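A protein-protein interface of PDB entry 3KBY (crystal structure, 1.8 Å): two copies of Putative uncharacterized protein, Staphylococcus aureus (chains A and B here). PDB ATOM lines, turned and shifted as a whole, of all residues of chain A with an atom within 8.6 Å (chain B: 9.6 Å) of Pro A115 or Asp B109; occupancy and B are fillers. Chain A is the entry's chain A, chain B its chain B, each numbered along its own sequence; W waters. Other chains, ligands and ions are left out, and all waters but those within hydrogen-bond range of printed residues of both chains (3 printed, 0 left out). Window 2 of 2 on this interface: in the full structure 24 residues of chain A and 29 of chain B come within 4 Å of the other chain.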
ATOM      1  N   TYR A  99      24.888 -32.682   3.182  1.00  0.00           N
ATOM      2  CA  TYR A  99      24.006 -31.637   3.689  1.00  0.00           C
ATOM      3  C   TYR A  99      23.562 -31.903   5.120  1.00  0.00           C
ATOM      4  O   TYR A  99      23.480 -30.961   5.911  1.00  0.00           O
ATOM      5  CB  TYR A  99      22.758 -31.477   2.836  1.00  0.00           C
ATOM      6  CG  TYR A  99      22.964 -31.111   1.382  1.00  0.00           C
ATOM      7  CD1 TYR A  99      24.096 -30.394   0.954  1.00  0.00           C
ATOM      8  CD2 TYR A  99      21.988 -31.443   0.443  1.00  0.00           C
ATOM      9  CE1 TYR A  99      24.262 -30.050  -0.401  1.00  0.00           C
ATOM     10  CE2 TYR A  99      22.142 -31.099  -0.908  1.00  0.00           C
ATOM     11  CZ  TYR A  99      23.274 -30.409  -1.313  1.00  0.00           C
ATOM     12  OH  TYR A  99      23.400 -30.079  -2.633  1.00  0.00           O
ATOM     13  N   ALA A 102      26.437 -31.200   7.389  1.00  0.00           N
ATOM     14  CA  ALA A 102      26.622 -29.759   7.479  1.00  0.00           C
ATOM     15  C   ALA A 102      25.514 -29.120   8.344  1.00  0.00           C
ATOM     16  O   ALA A 102      25.779 -28.202   9.111  1.00  0.00           O
ATOM     17  CB  ALA A 102      26.690 -29.144   6.078  1.00  0.00           C
ATOM     18  N   GLU A 106      25.870 -26.900  11.720  1.00  0.00           N
ATOM     19  CA  GLU A 106      25.201 -25.597  11.841  1.00  0.00           C
ATOM     20  C   GLU A 106      24.465 -25.416  13.166  1.00  0.00           C
ATOM     21  O   GLU A 106      24.360 -24.292  13.666  1.00  0.00           O
ATOM     22  CB  GLU A 106      24.292 -25.339  10.623  1.00  0.00           C
ATOM     23  CG  GLU A 106      25.094 -24.953   9.380  1.00  0.00           C
ATOM     24  CD  GLU A 106      24.541 -25.475   8.057  1.00  0.00           C
ATOM     25  OE1 GLU A 106      23.305 -25.619   7.921  1.00  0.00           O
ATOM     26  OE2 GLU A 106      25.365 -25.719   7.139  1.00  0.00           O
ATOM     27  N   ASN A 111      29.642 -23.326  10.235  1.00  0.00           N
ATOM     28  CA  ASN A 111      29.074 -23.284   8.891  1.00  0.00           C
ATOM     29  C   ASN A 111      30.143 -23.634   7.870  1.00  0.00           C
ATOM     30  O   ASN A 111      31.058 -22.840   7.611  1.00  0.00           O
ATOM     31  CB  ASN A 111      28.443 -21.908   8.633  1.00  0.00           C
ATOM     32  CG  ASN A 111      27.535 -21.465   9.782  1.00  0.00           C
ATOM     33  OD1 ASN A 111      26.506 -22.076  10.047  1.00  0.00           O
ATOM     34  ND2 ASN A 111      27.948 -20.430  10.497  1.00  0.00           N
ATOM     35  N   ILE A 112      30.053 -24.845   7.325  1.00  0.00           N
ATOM     36  CA  ILE A 112      31.086 -25.359   6.420  1.00  0.00           C
ATOM     37  C   ILE A 112      30.768 -25.123   4.939  1.00  0.00           C
ATOM     38  O   ILE A 112      31.677 -25.155   4.115  1.00  0.00           O
ATOM     39  CB  ILE A 112      31.409 -26.864   6.655  1.00  0.00           C
ATOM     40  CG1 ILE A 112      30.234 -27.754   6.222  1.00  0.00           C
ATOM     41  CG2 ILE A 112      31.835 -27.118   8.104  1.00  0.00           C
ATOM     42  CD1 ILE A 112      30.556 -29.243   6.232  1.00  0.00           C
ATOM     43  N   PHE A 113      29.492 -24.900   4.611  1.00  0.00           N
ATOM     44  CA  PHE A 113      29.063 -24.654   3.216  1.00  0.00           C
ATOM     45  C   PHE A 113      28.318 -23.345   3.077  1.00  0.00           C
ATOM     46  O   PHE A 113      27.673 -22.890   4.016  1.00  0.00           O
ATOM     47  CB  PHE A 113      28.075 -25.715   2.713  1.00  0.00           C
ATOM     48  CG  PHE A 113      28.632 -27.092   2.578  1.00  0.00           C
ATOM     49  CD1 PHE A 113      29.891 -27.319   2.027  1.00  0.00           C
ATOM     50  CD2 PHE A 113      27.852 -28.182   2.944  1.00  0.00           C
ATOM     51  CE1 PHE A 113      30.381 -28.622   1.897  1.00  0.00           C
ATOM     52  CE2 PHE A 113      28.322 -29.495   2.807  1.00  0.00           C
ATOM     53  CZ  PHE A 113      29.586 -29.713   2.276  1.00  0.00           C
ATOM     54  N   LYS A 114      28.374 -22.780   1.869  1.00  0.00           N
ATOM     55  CA  LYS A 114      27.515 -21.660   1.481  1.00  0.00           C
ATOM     56  C   LYS A 114      27.036 -21.918   0.051  1.00  0.00           C
ATOM     57  O   LYS A 114      27.860 -22.035  -0.859  1.00  0.00           O
ATOM     58  CB  LYS A 114      28.268 -20.326   1.550  1.00  0.00           C
ATOM     59  CG  LYS A 114      27.426 -19.100   1.123  1.00  0.00           C
ATOM     60  CD  LYS A 114      28.300 -17.937   0.653  1.00  0.00           C
ATOM     61  CE  LYS A 114      27.468 -16.716   0.263  1.00  0.00           C
ATOM     62  NZ  LYS A 114      26.782 -16.116   1.449  1.00  0.00           N
ATOM     63  N   PRO A 115      25.708 -22.041  -0.147  1.00  0.00           N
ATOM     64  CA  PRO A 115      24.654 -22.010   0.865  1.00  0.00           C
ATOM     65  C   PRO A 115      24.788 -23.127   1.916  1.00  0.00           C
ATOM     66  O   PRO A 115      25.472 -24.138   1.691  1.00  0.00           O
ATOM     67  CB  PRO A 115      23.383 -22.215   0.037  1.00  0.00           C
ATOM     68  CG  PRO A 115      23.749 -21.706  -1.317  1.00  0.00           C
ATOM     69  CD  PRO A 115      25.143 -22.178  -1.503  1.00  0.00           C
ATOM     70  N   SER A 116      24.130 -22.932   3.055  1.00  0.00           N
ATOM     71  CA  SER A 116      24.281 -23.822   4.208  1.00  0.00           C
ATOM     72  C   SER A 116      23.714 -25.217   3.952  1.00  0.00           C
ATOM     73  O   SER A 116      22.918 -25.429   3.017  1.00  0.00           O
ATOM     74  CB  SER A 116      23.580 -23.213   5.431  1.00  0.00           C
ATOM     75  OG  SER A 116      22.171 -23.262   5.243  1.00  0.00           O
ATOM     76  N   GLY A 117      24.111 -26.176   4.791  1.00  0.00           N
ATOM     77  CA  GLY A 117      23.569 -27.520   4.689  1.00  0.00           C
ATOM     78  C   GLY A 117      22.060 -27.540   4.892  1.00  0.00           C
ATOM     79  O   GLY A 117      21.349 -28.297   4.213  1.00  0.00           O
ATOM     80  N   PHE A 118      21.572 -26.702   5.807  1.00  0.00           N
ATOM     81  CA  PHE A 118      20.135 -26.572   6.047  1.00  0.00           C
ATOM     82  C   PHE A 118      19.404 -26.061   4.808  1.00  0.00           C
ATOM     83  O   PHE A 118      18.393 -26.639   4.395  1.00  0.00           O
ATOM     84  CB  PHE A 118      19.843 -25.659   7.241  1.00  0.00           C
ATOM     85  CG  PHE A 118      18.379 -25.357   7.421  1.00  0.00           C
ATOM     86  CD1 PHE A 118      17.490 -26.358   7.817  1.00  0.00           C
ATOM     87  CD2 PHE A 118      17.886 -24.068   7.206  1.00  0.00           C
ATOM     88  CE1 PHE A 118      16.139 -26.081   7.986  1.00  0.00           C
ATOM     89  CE2 PHE A 118      16.522 -23.790   7.369  1.00  0.00           C
ATOM     90  CZ  PHE A 118      15.659 -24.799   7.750  1.00  0.00           C
ATOM     91  N   THR A 119      19.928 -24.994   4.211  1.00  0.00           N
ATOM     92  CA  THR A 119      19.362 -24.448   2.978  1.00  0.00           C
ATOM     93  C   THR A 119      19.290 -25.498   1.865  1.00  0.00           C
ATOM     94  O   THR A 119      18.239 -25.699   1.251  1.00  0.00           O
ATOM     95  CB  THR A 119      20.180 -23.227   2.499  1.00  0.00           C
ATOM     96  OG1 THR A 119      20.036 -22.172   3.452  1.00  0.00           O
ATOM     97  CG2 THR A 119      19.712 -22.748   1.119  1.00  0.00           C
ATOM     98  N   MET A 120      20.408 -26.167   1.622  1.00  0.00           N
ATOM     99  CA  MET A 120      20.497 -27.131   0.530  1.00  0.00           C
ATOM    100  C   MET A 120      19.591 -28.334   0.808  1.00  0.00           C
ATOM    101  O   MET A 120      18.892 -28.810  -0.086  1.00  0.00           O
ATOM    102  CB  MET A 120      21.946 -27.553   0.288  1.00  0.00           C
ATOM    103  CG  MET A 120      22.875 -26.413  -0.122  1.00  0.00           C
ATOM    104  SD  MET A 120      22.268 -25.463  -1.724  1.00  0.00           S
ATOM    105  CE  MET A 120      22.470 -26.863  -3.088  1.00  0.00           C
ATOM    106  N   GLY A 121      19.601 -28.795   2.053  1.00  0.00           N
ATOM    107  CA  GLY A 121      18.752 -29.894   2.476  1.00  0.00           C
ATOM    108  C   GLY A 121      17.280 -29.605   2.253  1.00  0.00           C
ATOM    109  O   GLY A 121      16.542 -30.465   1.759  1.00  0.00           O
ATOM    110  N   MET A 122      16.856 -28.391   2.600  1.00  0.00           N
ATOM    111  CA  MET A 122      15.440 -28.011   2.500  1.00  0.00           C
ATOM    112  C   MET A 122      14.969 -27.853   1.048  1.00  0.00           C
ATOM    113  O   MET A 122      13.767 -27.801   0.790  1.00  0.00           O
ATOM    114  CB  MET A 122      15.155 -26.741   3.311  1.00  0.00           C
ATOM    115  CG  MET A 122      15.195 -26.956   4.837  1.00  0.00           C
ATOM    116  SD  MET A 122      14.085 -28.493   5.405  1.00  0.00           S
ATOM    117  CE  MET A 122      12.435 -27.957   4.529  1.00  0.00           C
ATOM    118  N   ASN A 123      15.917 -27.783   0.113  1.00  0.00           N
ATOM    119  CA  ASN A 123      15.597 -27.745  -1.314  1.00  0.00           C
ATOM    120  C   ASN A 123      15.835 -29.064  -2.061  1.00  0.00           C
ATOM    121  O   ASN A 123      15.599 -29.119  -3.270  1.00  0.00           O
ATOM    122  CB  ASN A 123      16.387 -26.621  -2.009  1.00  0.00           C
ATOM    123  CG  ASN A 123      15.872 -25.241  -1.628  1.00  0.00           C
ATOM    124  OD1 ASN A 123      14.962 -24.722  -2.265  1.00  0.00           O
ATOM    125  ND2 ASN A 123      16.409 -24.670  -0.550  1.00  0.00           N
ATOM    126  N   ILE B  51       7.562 -23.124  -1.298  1.00  0.00           N
ATOM    127  CA  ILE B  51       8.168 -22.120  -0.408  1.00  0.00           C
ATOM    128  C   ILE B  51       7.167 -21.041  -0.012  1.00  0.00           C
ATOM    129  O   ILE B  51       7.144 -20.591   1.138  1.00  0.00           O
ATOM    130  CB  ILE B  51       9.471 -21.510  -0.987  1.00  0.00           C
ATOM    131  CG1 ILE B  51      10.556 -22.585  -0.997  1.00  0.00           C
ATOM    132  CG2 ILE B  51       9.931 -20.292  -0.134  1.00  0.00           C
ATOM    133  CD1 ILE B  51      11.776 -22.258  -1.799  1.00  0.00           C
ATOM    134  N   TYR B  81      11.971  -7.495   5.941  1.00  0.00           N
ATOM    135  CA  TYR B  81      13.138  -6.629   5.730  1.00  0.00           C
ATOM    136  C   TYR B  81      12.966  -5.734   4.497  1.00  0.00           C
ATOM    137  O   TYR B  81      12.124  -5.993   3.637  1.00  0.00           O
ATOM    138  CB  TYR B  81      14.434  -7.461   5.607  1.00  0.00           C
ATOM    139  CG  TYR B  81      14.492  -8.339   4.378  1.00  0.00           C
ATOM    140  CD1 TYR B  81      15.115  -7.899   3.207  1.00  0.00           C
ATOM    141  CD2 TYR B  81      13.916  -9.616   4.382  1.00  0.00           C
ATOM    142  CE1 TYR B  81      15.157  -8.710   2.067  1.00  0.00           C
ATOM    143  CE2 TYR B  81      13.952 -10.431   3.260  1.00  0.00           C
ATOM    144  CZ  TYR B  81      14.572  -9.978   2.108  1.00  0.00           C
ATOM    145  OH  TYR B  81      14.603 -10.790   1.004  1.00  0.00           O
ATOM    146  N   VAL B 101      10.805 -17.274  11.397  1.00  0.00           N
ATOM    147  CA  VAL B 101      10.752 -16.493  10.150  1.00  0.00           C
ATOM    148  C   VAL B 101      12.127 -16.499   9.441  1.00  0.00           C
ATOM    149  O   VAL B 101      12.209 -16.676   8.217  1.00  0.00           O
ATOM    150  CB  VAL B 101      10.199 -15.058  10.401  1.00  0.00           C
ATOM    151  CG1 VAL B 101      10.381 -14.165   9.176  1.00  0.00           C
ATOM    152  CG2 VAL B 101       8.726 -15.138  10.737  1.00  0.00           C
ATOM    153  N   ALA B 102      13.188 -16.302  10.224  1.00  0.00           N
ATOM    154  CA  ALA B 102      14.550 -16.306   9.691  1.00  0.00           C
ATOM    155  C   ALA B 102      14.934 -17.679   9.102  1.00  0.00           C
ATOM    156  O   ALA B 102      15.526 -17.750   8.008  1.00  0.00           O
ATOM    157  CB  ALA B 102      15.541 -15.873  10.774  1.00  0.00           C
ATOM    158  N   ALA B 103      14.603 -18.759   9.814  1.00  0.00           N
ATOM    159  CA  ALA B 103      14.834 -20.113   9.279  1.00  0.00           C
ATOM    160  C   ALA B 103      14.119 -20.344   7.946  1.00  0.00           C
ATOM    161  O   ALA B 103      14.687 -20.935   7.031  1.00  0.00           O
ATOM    162  CB  ALA B 103      14.427 -21.175  10.286  1.00  0.00           C
ATOM    163  N   ALA B 104      12.880 -19.861   7.832  1.00  0.00           N
ATOM    164  CA  ALA B 104      12.125 -19.977   6.573  1.00  0.00           C
ATOM    165  C   ALA B 104      12.800 -19.188   5.441  1.00  0.00           C
ATOM    166  O   ALA B 104      12.913 -19.664   4.302  1.00  0.00           O
ATOM    167  CB  ALA B 104      10.674 -19.500   6.783  1.00  0.00           C
ATOM    168  N   LEU B 105      13.260 -17.984   5.760  1.00  0.00           N
ATOM    169  CA  LEU B 105      13.998 -17.173   4.798  1.00  0.00           C
ATOM    170  C   LEU B 105      15.295 -17.855   4.389  1.00  0.00           C
ATOM    171  O   LEU B 105      15.699 -17.768   3.225  1.00  0.00           O
ATOM    172  CB  LEU B 105      14.254 -15.745   5.316  1.00  0.00           C
ATOM    173  CG  LEU B 105      12.986 -14.867   5.302  1.00  0.00           C
ATOM    174  CD1 LEU B 105      13.203 -13.565   6.061  1.00  0.00           C
ATOM    175  CD2 LEU B 105      12.532 -14.580   3.853  1.00  0.00           C
ATOM    176  N   GLU B 106      15.913 -18.577   5.322  1.00  0.00           N
ATOM    177  CA  GLU B 106      17.145 -19.322   5.020  1.00  0.00           C
ATOM    178  C   GLU B 106      16.943 -20.434   3.986  1.00  0.00           C
ATOM    179  O   GLU B 106      17.877 -20.770   3.248  1.00  0.00           O
ATOM    180  CB  GLU B 106      17.817 -19.826   6.312  1.00  0.00           C
ATOM    181  CG  GLU B 106      18.481 -18.689   7.088  1.00  0.00           C
ATOM    182  CD  GLU B 106      18.497 -18.860   8.604  1.00  0.00           C
ATOM    183  OE1 GLU B 106      18.415 -20.009   9.127  1.00  0.00           O
ATOM    184  OE2 GLU B 106      18.619 -17.806   9.280  1.00  0.00           O
ATOM    185  N   VAL B 107      15.720 -20.958   3.888  1.00  0.00           N
ATOM    186  CA  VAL B 107      15.373 -21.942   2.855  1.00  0.00           C
ATOM    187  C   VAL B 107      15.541 -21.348   1.441  1.00  0.00           C
ATOM    188  O   VAL B 107      15.896 -22.060   0.486  1.00  0.00           O
ATOM    189  CB  VAL B 107      13.928 -22.494   3.045  1.00  0.00           C
ATOM    190  CG1 VAL B 107      13.542 -23.437   1.904  1.00  0.00           C
ATOM    191  CG2 VAL B 107      13.800 -23.226   4.385  1.00  0.00           C
ATOM    192  N   THR B 108      15.308 -20.042   1.315  1.00  0.00           N
ATOM    193  CA  THR B 108      15.508 -19.343   0.032  1.00  0.00           C
ATOM    194  C   THR B 108      16.883 -18.680  -0.066  1.00  0.00           C
ATOM    195  O   THR B 108      17.108 -17.838  -0.946  1.00  0.00           O
ATOM    196  CB  THR B 108      14.428 -18.256  -0.224  1.00  0.00           C
ATOM    197  OG1 THR B 108      14.444 -17.287   0.835  1.00  0.00           O
ATOM    198  CG2 THR B 108      13.045 -18.863  -0.331  1.00  0.00           C
ATOM    199  N   ASP B 109      17.776 -19.046   0.852  1.00  0.00           N
ATOM    200  CA  ASP B 109      19.143 -18.517   0.922  1.00  0.00           C
ATOM    201  C   ASP B 109      19.168 -17.006   1.150  1.00  0.00           C
ATOM    202  O   ASP B 109      20.025 -16.295   0.610  1.00  0.00           O
ATOM    203  CB  ASP B 109      19.950 -18.927  -0.317  1.00  0.00           C
ATOM    204  CG  ASP B 109      21.452 -18.751  -0.131  1.00  0.00           C
ATOM    205  OD1 ASP B 109      21.960 -18.842   1.020  1.00  0.00           O
ATOM    206  OD2 ASP B 109      22.126 -18.511  -1.150  1.00  0.00           O
ATOM    207  N   VAL B 110      18.207 -16.527   1.944  1.00  0.00           N
ATOM    208  CA  VAL B 110      18.221 -15.162   2.470  1.00  0.00           C
ATOM    209  C   VAL B 110      18.595 -15.276   3.943  1.00  0.00           C
ATOM    210  O   VAL B 110      17.871 -15.894   4.720  1.00  0.00           O
ATOM    211  CB  VAL B 110      16.850 -14.460   2.309  1.00  0.00           C
ATOM    212  CG1 VAL B 110      16.868 -13.104   3.004  1.00  0.00           C
ATOM    213  CG2 VAL B 110      16.549 -14.254   0.833  1.00  0.00           C
ATOM    214  N   ASN B 111      19.733 -14.699   4.321  1.00  0.00           N
ATOM    215  CA  ASN B 111      20.270 -14.912   5.665  1.00  0.00           C
ATOM    216  C   ASN B 111      20.339 -13.621   6.468  1.00  0.00           C
ATOM    217  O   ASN B 111      21.248 -12.813   6.295  1.00  0.00           O
ATOM    218  CB  ASN B 111      21.627 -15.628   5.604  1.00  0.00           C
ATOM    219  CG  ASN B 111      21.577 -16.879   4.749  1.00  0.00           C
ATOM    220  OD1 ASN B 111      20.985 -17.899   5.134  1.00  0.00           O
ATOM    221  ND2 ASN B 111      22.169 -16.801   3.566  1.00  0.00           N
ATOM    222  N   ILE B 112      19.359 -13.424   7.340  1.00  0.00           N
ATOM    223  CA  ILE B 112      19.212 -12.141   8.020  1.00  0.00           C
ATOM    224  C   ILE B 112      19.850 -12.077   9.417  1.00  0.00           C
ATOM    225  O   ILE B 112      20.125 -10.973   9.913  1.00  0.00           O
ATOM    226  CB  ILE B 112      17.730 -11.646   8.058  1.00  0.00           C
ATOM    227  CG1 ILE B 112      16.857 -12.534   8.946  1.00  0.00           C
ATOM    228  CG2 ILE B 112      17.161 -11.544   6.643  1.00  0.00           C
ATOM    229  CD1 ILE B 112      15.451 -11.942   9.191  1.00  0.00           C
ATOM    230  N   TYR B 136       6.046 -26.909   9.055  1.00  0.00           N
ATOM    231  CA  TYR B 136       6.584 -26.041   8.000  1.00  0.00           C
ATOM    232  C   TYR B 136       7.485 -26.807   7.015  1.00  0.00           C
ATOM    233  O   TYR B 136       7.276 -26.748   5.794  1.00  0.00           O
ATOM    234  CB  TYR B 136       7.341 -24.821   8.614  1.00  0.00           C
ATOM    235  CG  TYR B 136       8.178 -24.069   7.596  1.00  0.00           C
ATOM    236  CD1 TYR B 136       7.594 -23.134   6.750  1.00  0.00           C
ATOM    237  CD2 TYR B 136       9.547 -24.320   7.456  1.00  0.00           C
ATOM    238  CE1 TYR B 136       8.360 -22.444   5.780  1.00  0.00           C
ATOM    239  CE2 TYR B 136      10.326 -23.645   6.515  1.00  0.00           C
ATOM    240  CZ  TYR B 136       9.735 -22.713   5.674  1.00  0.00           C
ATOM    241  OH  TYR B 136      10.495 -22.048   4.720  1.00  0.00           O
HETATM  242  O   HOH W   1      21.577 -20.442   6.046  1.00  0.00           O
HETATM  243  O   HOH W   2      22.324 -20.575   3.279  1.00  0.00           O
HETATM  244  O   HOH W   3      14.884 -21.941  -2.769  1.00  0.00           O
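O of Glu B106 sits at hydrogen-bond distance from OG1 of Thr A119 (2.6 Å).
ND2 of Asn A123 lies within hydrogen-bond range of O of Val B107, at 2.9 Å.
The side-chain carboxylate of Glu A106 sits at hydrogen-bond distance from the backbone NH of Phe A118 (2.9 Å).
OG of Ser A116 sits at hydrogen-bond distance from OG1 of Thr A119 (3.0 Å).
The side-chain amide nitrogen (ND2) of Asn A123 lies within hydrogen-bond range of the backbone carbonyl oxygen (O) of Thr A119 (2.8 Å).
The side-chain carboxylate (OD1) of Asp B109 lies within hydrogen-bond range of the side-chain amide nitrogen (ND2) of Asn B111 (3.3 Å).
Among the printed residues, merely in contact across the chains: Pro A115 with Asp B109, Phe A118 with Ala B103, Thr A119 with Val B107 and Met A122 with Val B107.
Of chain B, only Asp B109 comes within 4 Å of Pro A115.
Of the printed residues of chain B, Met A122 touches Val B107.
Of the printed residues of chain B, Thr A119 touches Glu B106 and Val B107.
Of the printed residues of chain B, Asn A123 touches Val B107 (2.9 Å).
Of the printed residues of chain B, Phe A118 touches Ala B103.
Of the printed residues of chain A, Ala B103 touches Phe A118 (3.4 Å).
The nearest residue of chain A that does not touch Asp B109 is Thr A119 (4.1 Å).
Hydrophobic or aromatic side chains of chain B within 4 Å of the printed part of chain A: Val B107.
4 positions are printed for both chains.
Of the 6 pairs that touch across the chains among the printed residues, none has its exchanged pair printed and touching as well.
Water W1 lies within hydrogen-bond range of the side-chain amide oxygen (OD1) of Asn B111, the side-chain hydroxyl (OG) of Ser A116 and the side-chain hydroxyl (OG1) of Thr A119.
Water W2 lies within hydrogen-bond range of OG1 of Thr A119 (2.8 Å), OD1 of Asp B109 (2.9 Å) and N of Ser A116 (3.0 Å).
Water W3 bridges OD1 of Asn A123 and O of Val B107.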
